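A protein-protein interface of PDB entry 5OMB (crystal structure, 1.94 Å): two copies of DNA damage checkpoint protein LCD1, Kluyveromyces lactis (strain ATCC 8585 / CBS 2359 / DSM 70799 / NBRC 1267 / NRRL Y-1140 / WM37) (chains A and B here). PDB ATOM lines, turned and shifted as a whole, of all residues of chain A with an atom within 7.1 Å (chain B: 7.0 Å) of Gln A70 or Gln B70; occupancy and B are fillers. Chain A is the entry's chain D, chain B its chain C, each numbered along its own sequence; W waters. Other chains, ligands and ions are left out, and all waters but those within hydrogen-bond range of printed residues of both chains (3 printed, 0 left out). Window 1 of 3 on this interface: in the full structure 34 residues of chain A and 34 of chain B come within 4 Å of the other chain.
Gln B70 touches Gln A70. Gln A70 touches Leu B73. Gln B70 touches Leu A73. Glu B74 touches Leu A73.
His A66 touches Asp B67, and with the chains exchanged Asp A67 touches His B66. Gln B70 touches its own counterpart, Gln A70. Gln A70 touches Leu B73, and with the chains exchanged Leu A73 touches Gln B70. Leu A73 touches Glu B74, but with the chains exchanged Glu A74 does not touch Leu B73 (5.2 Å). Of the 6 pairs that touch across the chains among the printed residues, 5 have their exchanged pair printed and touching as well.
Water W2 bridges OE1 of Gln B70 (2.6 Å) and O of His A66 (2.7 Å). Water W1 bridges the backbone carbonyl oxygen of His B66 and the side-chain amide nitrogen of Gln A70. Water W3 lies within hydrogen-bond range of NE2 of Gln A70 (2.8 Å), O of His B66 (3.1 Å) and OD1 of Asp A67 (3.2 Å).
Hydrophobic or aromatic side chains of chain B that line the printed part of chain A: His B66 and Leu B73. Of the 12 printed residues of chain A, 4 touch a printed residue of chain B. Among the printed residues, 6 pairs touch across the chains.
Of the printed residues of chain B, Gln A70 touches Gln B70 and Leu B73. Of chain A, only Gln A70 and Leu A73 come within 4 Å of Gln B70. Of the printed residues of chain A, Asp B67 touches His A66. Of the printed residues of chain B, His A66 touches Asp B67. Ser B75 touches none of the printed residues of chain A.
The side-chain carboxylate (OD1) of Asp B67 lies within hydrogen-bond range of a ring nitrogen (ND1) of His A66 (2.7 Å). ND1 of His B66 sits at hydrogen-bond distance from OD1 of Asp A67, at 2.7 Å.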
ATOM      1  N   ARG A  64      -1.760 -27.479   0.247  1.00  0.00           N
ATOM      2  CA  ARG A  64      -1.219 -26.141  -0.026  1.00  0.00           C
ATOM      3  C   ARG A  64      -1.495 -25.183   1.148  1.00  0.00           C
ATOM      4  O   ARG A  64      -0.593 -24.440   1.557  1.00  0.00           O
ATOM      5  CB  ARG A  64      -1.841 -25.588  -1.317  1.00  0.00           C
ATOM      6  CG  ARG A  64      -0.989 -24.580  -2.079  1.00  0.00           C
ATOM      7  CD  ARG A  64      -1.057 -24.786  -3.592  1.00  0.00           C
ATOM      8  NE  ARG A  64      -2.432 -24.872  -4.093  1.00  0.00           N
ATOM      9  CZ  ARG A  64      -2.940 -25.929  -4.724  1.00  0.00           C
ATOM     10  NH1 ARG A  64      -2.184 -26.993  -4.971  1.00  0.00           N
ATOM     11  NH2 ARG A  64      -4.204 -25.922  -5.124  1.00  0.00           N
ATOM     12  N   GLU A  65      -2.734 -25.220   1.700  1.00  0.00           N
ATOM     13  CA  GLU A  65      -3.157 -24.396   2.836  1.00  0.00           C
ATOM     14  C   GLU A  65      -2.363 -24.770   4.073  1.00  0.00           C
ATOM     15  O   GLU A  65      -1.784 -23.890   4.712  1.00  0.00           O
ATOM     16  CB  GLU A  65      -4.656 -24.543   3.101  1.00  0.00           C
ATOM     17  CG  GLU A  65      -5.533 -23.803   2.102  1.00  0.00           C
ATOM     18  CD  GLU A  65      -7.038 -23.960   2.257  1.00  0.00           C
ATOM     19  OE1 GLU A  65      -7.490 -24.660   3.193  1.00  0.00           O
ATOM     20  OE2 GLU A  65      -7.770 -23.368   1.430  1.00  0.00           O
ATOM     21  N   HIS A  66      -2.251 -26.081   4.357  1.00  0.00           N
ATOM     22  CA  HIS A  66      -1.488 -26.580   5.491  1.00  0.00           C
ATOM     23  C   HIS A  66      -0.007 -26.123   5.456  1.00  0.00           C
ATOM     24  O   HIS A  66       0.483 -25.606   6.465  1.00  0.00           O
ATOM     25  CB  HIS A  66      -1.640 -28.101   5.628  1.00  0.00           C
ATOM     26  CG  HIS A  66      -2.966 -28.548   6.194  1.00  0.00           C
ATOM     27  ND1 HIS A  66      -3.059 -29.671   7.005  1.00  0.00           N
ATOM     28  CD2 HIS A  66      -4.208 -28.025   6.037  1.00  0.00           C
ATOM     29  CE1 HIS A  66      -4.341 -29.787   7.321  1.00  0.00           C
ATOM     30  NE2 HIS A  66      -5.070 -28.814   6.769  1.00  0.00           N
ATOM     31  N   ASP A  67       0.675 -26.265   4.292  1.00  0.00           N
ATOM     32  CA  ASP A  67       2.069 -25.841   4.106  1.00  0.00           C
ATOM     33  C   ASP A  67       2.265 -24.345   4.327  1.00  0.00           C
ATOM     34  O   ASP A  67       3.241 -23.944   4.973  1.00  0.00           O
ATOM     35  CB  ASP A  67       2.618 -26.300   2.745  1.00  0.00           C
ATOM     36  CG  ASP A  67       2.707 -27.812   2.631  1.00  0.00           C
ATOM     37  OD1 ASP A  67       2.408 -28.503   3.634  1.00  0.00           O
ATOM     38  OD2 ASP A  67       3.068 -28.307   1.538  1.00  0.00           O
ATOM     39  N   ASP A  68       1.312 -23.532   3.839  1.00  0.00           N
ATOM     40  CA  ASP A  68       1.296 -22.087   4.011  1.00  0.00           C
ATOM     41  C   ASP A  68       1.114 -21.726   5.495  1.00  0.00           C
ATOM     42  O   ASP A  68       1.829 -20.858   5.986  1.00  0.00           O
ATOM     43  CB  ASP A  68       0.202 -21.443   3.141  1.00  0.00           C
ATOM     44  CG  ASP A  68       0.481 -21.457   1.639  1.00  0.00           C
ATOM     45  OD1 ASP A  68      -0.403 -21.009   0.863  1.00  0.00           O
ATOM     46  OD2 ASP A  68       1.567 -21.947   1.233  1.00  0.00           O
ATOM     47  N   ASN A  69       0.182 -22.406   6.202  1.00  0.00           N
ATOM     48  CA  ASN A  69      -0.090 -22.223   7.639  1.00  0.00           C
ATOM     49  C   ASN A  69       1.141 -22.597   8.457  1.00  0.00           C
ATOM     50  O   ASN A  69       1.462 -21.878   9.406  1.00  0.00           O
ATOM     51  CB  ASN A  69      -1.275 -23.065   8.087  1.00  0.00           C
ATOM     52  CG  ASN A  69      -2.459 -22.254   8.491  1.00  0.00           C
ATOM     53  OD1 ASN A  69      -3.184 -21.717   7.644  1.00  0.00           O
ATOM     54  ND2 ASN A  69      -2.686 -22.160   9.801  1.00  0.00           N
ATOM     55  N   GLN A  70       1.837 -23.705   8.075  1.00  0.00           N
ATOM     56  CA  GLN A  70       3.069 -24.176   8.708  1.00  0.00           C
ATOM     57  C   GLN A  70       4.141 -23.066   8.635  1.00  0.00           C
ATOM     58  O   GLN A  70       4.827 -22.824   9.635  1.00  0.00           O
ATOM     59  CB  GLN A  70       3.596 -25.455   8.040  1.00  0.00           C
ATOM     60  CG  GLN A  70       4.785 -26.089   8.785  1.00  0.00           C
ATOM     61  CD  GLN A  70       5.583 -27.125   8.012  1.00  0.00           C
ATOM     62  OE1 GLN A  70       6.635 -27.586   8.471  1.00  0.00           O
ATOM     63  NE2 GLN A  70       5.117 -27.531   6.832  1.00  0.00           N
ATOM     64  N   LYS A  71       4.247 -22.388   7.462  1.00  0.00           N
ATOM     65  CA  LYS A  71       5.192 -21.295   7.209  1.00  0.00           C
ATOM     66  C   LYS A  71       4.864 -20.034   8.016  1.00  0.00           C
ATOM     67  O   LYS A  71       5.770 -19.444   8.601  1.00  0.00           O
ATOM     68  CB  LYS A  71       5.321 -21.001   5.701  1.00  0.00           C
ATOM     69  CG  LYS A  71       6.256 -21.986   4.992  1.00  0.00           C
ATOM     70  CD  LYS A  71       5.983 -22.107   3.491  1.00  0.00           C
ATOM     71  CE  LYS A  71       6.953 -21.305   2.657  1.00  0.00           C
ATOM     72  NZ  LYS A  71       6.704 -21.477   1.201  1.00  0.00           N
ATOM     73  N   LYS A  72       3.578 -19.647   8.071  1.00  0.00           N
ATOM     74  CA  LYS A  72       3.093 -18.482   8.817  1.00  0.00           C
ATOM     75  C   LYS A  72       3.238 -18.637  10.340  1.00  0.00           C
ATOM     76  O   LYS A  72       3.593 -17.666  11.014  1.00  0.00           O
ATOM     77  CB  LYS A  72       1.658 -18.125   8.425  1.00  0.00           C
ATOM     78  CG  LYS A  72       1.557 -17.548   7.016  1.00  0.00           C
ATOM     79  CD  LYS A  72       0.110 -17.458   6.534  1.00  0.00           C
ATOM     80  CE  LYS A  72       0.003 -17.023   5.089  1.00  0.00           C
ATOM     81  NZ  LYS A  72       0.360 -18.116   4.141  1.00  0.00           N
ATOM     82  N   LEU A  73       2.969 -19.853  10.868  1.00  0.00           N
ATOM     83  CA  LEU A  73       3.110 -20.197  12.286  1.00  0.00           C
ATOM     84  C   LEU A  73       4.590 -20.165  12.662  1.00  0.00           C
ATOM     85  O   LEU A  73       4.926 -19.649  13.731  1.00  0.00           O
ATOM     86  CB  LEU A  73       2.495 -21.583  12.597  1.00  0.00           C
ATOM     87  CG  LEU A  73       2.973 -22.308  13.877  1.00  0.00           C
ATOM     88  CD1 LEU A  73       2.089 -21.989  15.060  1.00  0.00           C
ATOM     89  CD2 LEU A  73       3.048 -23.812  13.670  1.00  0.00           C
ATOM     90  N   GLU A  74       5.462 -20.727  11.801  1.00  0.00           N
ATOM     91  CA  GLU A  74       6.906 -20.754  12.021  1.00  0.00           C
ATOM     92  C   GLU A  74       7.467 -19.323  12.094  1.00  0.00           C
ATOM     93  O   GLU A  74       8.241 -19.022  13.006  1.00  0.00           O
ATOM     94  CB  GLU A  74       7.609 -21.553  10.922  1.00  0.00           C
ATOM     95  CG  GLU A  74       9.030 -21.962  11.257  1.00  0.00           C
ATOM     96  CD  GLU A  74       9.682 -22.827  10.199  1.00  0.00           C
ATOM     97  OE1 GLU A  74       9.262 -23.998  10.047  1.00  0.00           O
ATOM     98  OE2 GLU A  74      10.612 -22.335   9.520  1.00  0.00           O
ATOM     99  N   SER A  75       7.034 -18.448  11.161  1.00  0.00           N
ATOM    100  CA  SER A  75       7.456 -17.050  11.051  1.00  0.00           C
ATOM    101  C   SER A  75       7.021 -16.236  12.278  1.00  0.00           C
ATOM    102  O   SER A  75       7.825 -15.463  12.805  1.00  0.00           O
ATOM    103  CB  SER A  75       6.930 -16.434   9.755  1.00  0.00           C
ATOM    104  OG  SER A  75       7.013 -15.019   9.743  1.00  0.00           O
ATOM    105  N   ARG B  64      -1.083 -36.241   6.014  1.00  0.00           N
ATOM    106  CA  ARG B  64      -0.876 -36.727   7.388  1.00  0.00           C
ATOM    107  C   ARG B  64       0.609 -36.582   7.790  1.00  0.00           C
ATOM    108  O   ARG B  64       0.914 -36.290   8.959  1.00  0.00           O
ATOM    109  CB  ARG B  64      -1.306 -38.201   7.550  1.00  0.00           C
ATOM    110  CG  ARG B  64      -2.754 -38.515   7.146  1.00  0.00           C
ATOM    111  CD  ARG B  64      -3.808 -38.110   8.170  1.00  0.00           C
ATOM    112  NE  ARG B  64      -5.113 -37.875   7.539  1.00  0.00           N
ATOM    113  CZ  ARG B  64      -6.015 -38.821   7.283  1.00  0.00           C
ATOM    114  NH1 ARG B  64      -5.771 -40.088   7.599  1.00  0.00           N
ATOM    115  NH2 ARG B  64      -7.167 -38.506   6.704  1.00  0.00           N
ATOM    116  N   GLU B  65       1.518 -36.787   6.806  1.00  0.00           N
ATOM    117  CA  GLU B  65       2.972 -36.699   6.985  1.00  0.00           C
ATOM    118  C   GLU B  65       3.384 -35.275   7.227  1.00  0.00           C
ATOM    119  O   GLU B  65       4.126 -35.018   8.173  1.00  0.00           O
ATOM    120  CB  GLU B  65       3.738 -37.324   5.805  1.00  0.00           C
ATOM    121  CG  GLU B  65       3.731 -38.841   5.852  1.00  0.00           C
ATOM    122  CD  GLU B  65       4.343 -39.586   4.678  1.00  0.00           C
ATOM    123  OE1 GLU B  65       4.700 -38.945   3.662  1.00  0.00           O
ATOM    124  OE2 GLU B  65       4.453 -40.830   4.779  1.00  0.00           O
ATOM    125  N   HIS B  66       2.830 -34.341   6.433  1.00  0.00           N
ATOM    126  CA  HIS B  66       3.053 -32.903   6.565  1.00  0.00           C
ATOM    127  C   HIS B  66       2.528 -32.386   7.912  1.00  0.00           C
ATOM    128  O   HIS B  66       3.156 -31.505   8.510  1.00  0.00           O
ATOM    129  CB  HIS B  66       2.398 -32.148   5.400  1.00  0.00           C
ATOM    130  CG  HIS B  66       3.216 -32.155   4.138  1.00  0.00           C
ATOM    131  ND1 HIS B  66       3.347 -31.020   3.364  1.00  0.00           N
ATOM    132  CD2 HIS B  66       3.933 -33.153   3.570  1.00  0.00           C
ATOM    133  CE1 HIS B  66       4.125 -31.355   2.352  1.00  0.00           C
ATOM    134  NE2 HIS B  66       4.510 -32.627   2.433  1.00  0.00           N
ATOM    135  N   ASP B  67       1.387 -32.922   8.389  1.00  0.00           N
ATOM    136  CA  ASP B  67       0.818 -32.520   9.675  1.00  0.00           C
ATOM    137  C   ASP B  67       1.684 -33.016  10.830  1.00  0.00           C
ATOM    138  O   ASP B  67       1.942 -32.257  11.771  1.00  0.00           O
ATOM    139  CB  ASP B  67      -0.642 -32.966   9.818  1.00  0.00           C
ATOM    140  CG  ASP B  67      -1.624 -32.179   8.959  1.00  0.00           C
ATOM    141  OD1 ASP B  67      -1.241 -31.102   8.451  1.00  0.00           O
ATOM    142  OD2 ASP B  67      -2.781 -32.631   8.815  1.00  0.00           O
ATOM    143  N   ASP B  68       2.178 -34.260  10.719  1.00  0.00           N
ATOM    144  CA  ASP B  68       3.074 -34.915  11.675  1.00  0.00           C
ATOM    145  C   ASP B  68       4.394 -34.159  11.760  1.00  0.00           C
ATOM    146  O   ASP B  68       4.905 -33.922  12.866  1.00  0.00           O
ATOM    147  CB  ASP B  68       3.364 -36.350  11.219  1.00  0.00           C
ATOM    148  CG  ASP B  68       3.018 -37.396  12.245  1.00  0.00           C
ATOM    149  OD1 ASP B  68       3.853 -37.637  13.145  1.00  0.00           O
ATOM    150  OD2 ASP B  68       1.920 -37.993  12.138  1.00  0.00           O
ATOM    151  N   ASN B  69       4.949 -33.789  10.586  1.00  0.00           N
ATOM    152  CA  ASN B  69       6.203 -33.075  10.503  1.00  0.00           C
ATOM    153  C   ASN B  69       6.119 -31.670  11.059  1.00  0.00           C
ATOM    154  O   ASN B  69       7.106 -31.203  11.637  1.00  0.00           O
ATOM    155  CB  ASN B  69       6.755 -33.092   9.106  1.00  0.00           C
ATOM    156  CG  ASN B  69       7.993 -33.938   9.025  1.00  0.00           C
ATOM    157  OD1 ASN B  69       9.118 -33.455   9.234  1.00  0.00           O
ATOM    158  ND2 ASN B  69       7.805 -35.234   8.779  1.00  0.00           N
ATOM    159  N   GLN B  70       4.946 -31.006  10.918  1.00  0.00           N
ATOM    160  CA  GLN B  70       4.730 -29.674  11.460  1.00  0.00           C
ATOM    161  C   GLN B  70       4.808 -29.757  12.991  1.00  0.00           C
ATOM    162  O   GLN B  70       5.549 -28.976  13.592  1.00  0.00           O
ATOM    163  CB  GLN B  70       3.393 -29.064  10.994  1.00  0.00           C
ATOM    164  CG  GLN B  70       2.957 -27.843  11.824  1.00  0.00           C
ATOM    165  CD  GLN B  70       1.791 -27.075  11.260  1.00  0.00           C
ATOM    166  OE1 GLN B  70       1.503 -27.122  10.067  1.00  0.00           O
ATOM    167  NE2 GLN B  70       1.121 -26.296  12.099  1.00  0.00           N
ATOM    168  N   LYS B  71       4.071 -30.724  13.605  1.00  0.00           N
ATOM    169  CA  LYS B  71       4.051 -30.947  15.059  1.00  0.00           C
ATOM    170  C   LYS B  71       5.465 -31.221  15.621  1.00  0.00           C
ATOM    171  O   LYS B  71       5.836 -30.640  16.640  1.00  0.00           O
ATOM    172  CB  LYS B  71       3.060 -32.059  15.429  1.00  0.00           C
ATOM    173  CG  LYS B  71       1.605 -31.623  15.293  1.00  0.00           C
ATOM    174  CD  LYS B  71       0.632 -32.801  15.408  1.00  0.00           C
ATOM    175  CE  LYS B  71      -0.807 -32.405  15.161  1.00  0.00           C
ATOM    176  NZ  LYS B  71      -1.100 -32.217  13.711  1.00  0.00           N
ATOM    177  N   LYS B  72       6.258 -32.039  14.913  1.00  0.00           N
ATOM    178  CA  LYS B  72       7.640 -32.386  15.241  1.00  0.00           C
ATOM    179  C   LYS B  72       8.533 -31.123  15.205  1.00  0.00           C
ATOM    180  O   LYS B  72       9.234 -30.843  16.187  1.00  0.00           O
ATOM    181  CB  LYS B  72       8.167 -33.437  14.246  1.00  0.00           C
ATOM    182  CG  LYS B  72       9.494 -34.074  14.643  1.00  0.00           C
ATOM    183  CD  LYS B  72       9.995 -35.069  13.601  1.00  0.00           C
ATOM    184  CE  LYS B  72      11.154 -35.895  14.117  1.00  0.00           C
ATOM    185  NZ  LYS B  72      11.661 -36.844  13.088  1.00  0.00           N
ATOM    186  N   LEU B  73       8.500 -30.370  14.073  1.00  0.00           N
ATOM    187  CA  LEU B  73       9.301 -29.160  13.884  1.00  0.00           C
ATOM    188  C   LEU B  73       8.934 -28.039  14.870  1.00  0.00           C
ATOM    189  O   LEU B  73       9.833 -27.400  15.397  1.00  0.00           O
ATOM    190  CB  LEU B  73       9.272 -28.666  12.428  1.00  0.00           C
ATOM    191  CG  LEU B  73       9.886 -29.610  11.378  1.00  0.00           C
ATOM    192  CD1 LEU B  73       9.434 -29.236   9.969  1.00  0.00           C
ATOM    193  CD2 LEU B  73      11.406 -29.655  11.463  1.00  0.00           C
ATOM    194  N   GLU B  74       7.641 -27.836  15.152  1.00  0.00           N
ATOM    195  CA  GLU B  74       7.168 -26.835  16.109  1.00  0.00           C
ATOM    196  C   GLU B  74       7.634 -27.178  17.554  1.00  0.00           C
ATOM    197  O   GLU B  74       8.030 -26.277  18.303  1.00  0.00           O
ATOM    198  CB  GLU B  74       5.650 -26.715  16.023  1.00  0.00           C
ATOM    199  CG  GLU B  74       5.043 -25.584  16.832  1.00  0.00           C
ATOM    200  CD  GLU B  74       3.563 -25.747  17.126  1.00  0.00           C
ATOM    201  OE1 GLU B  74       2.839 -26.336  16.289  1.00  0.00           O
ATOM    202  OE2 GLU B  74       3.125 -25.276  18.200  1.00  0.00           O
ATOM    203  N   SER B  75       7.623 -28.479  17.909  1.00  0.00           N
ATOM    204  CA  SER B  75       8.062 -29.007  19.199  1.00  0.00           C
ATOM    205  C   SER B  75       9.569 -28.758  19.377  1.00  0.00           C
ATOM    206  O   SER B  75      10.004 -28.345  20.456  1.00  0.00           O
ATOM    207  CB  SER B  75       7.762 -30.501  19.288  1.00  0.00           C
ATOM    208  OG  SER B  75       8.113 -31.024  20.559  1.00  0.00           O
ATOM    209  N   SER B  76      10.333 -28.998  18.301  1.00  0.00           N
ATOM    210  CA  SER B  76      11.777 -28.834  18.177  1.00  0.00           C
ATOM    211  C   SER B  76      12.133 -27.354  18.265  1.00  0.00           C
ATOM    212  O   SER B  76      13.092 -27.005  18.955  1.00  0.00           O
ATOM    213  CB  SER B  76      12.251 -29.427  16.850  1.00  0.00           C
ATOM    214  OG  SER B  76      13.616 -29.157  16.578  1.00  0.00           O
HETATM  215  O   HOH W   1       5.241 -30.281   7.343  1.00  0.00           O
HETATM  216  O   HOH W   2      -0.690 -26.332   8.841  1.00  0.00           O
HETATM  217  O   HOH W   3       2.734 -29.016   6.736  1.00  0.00           O
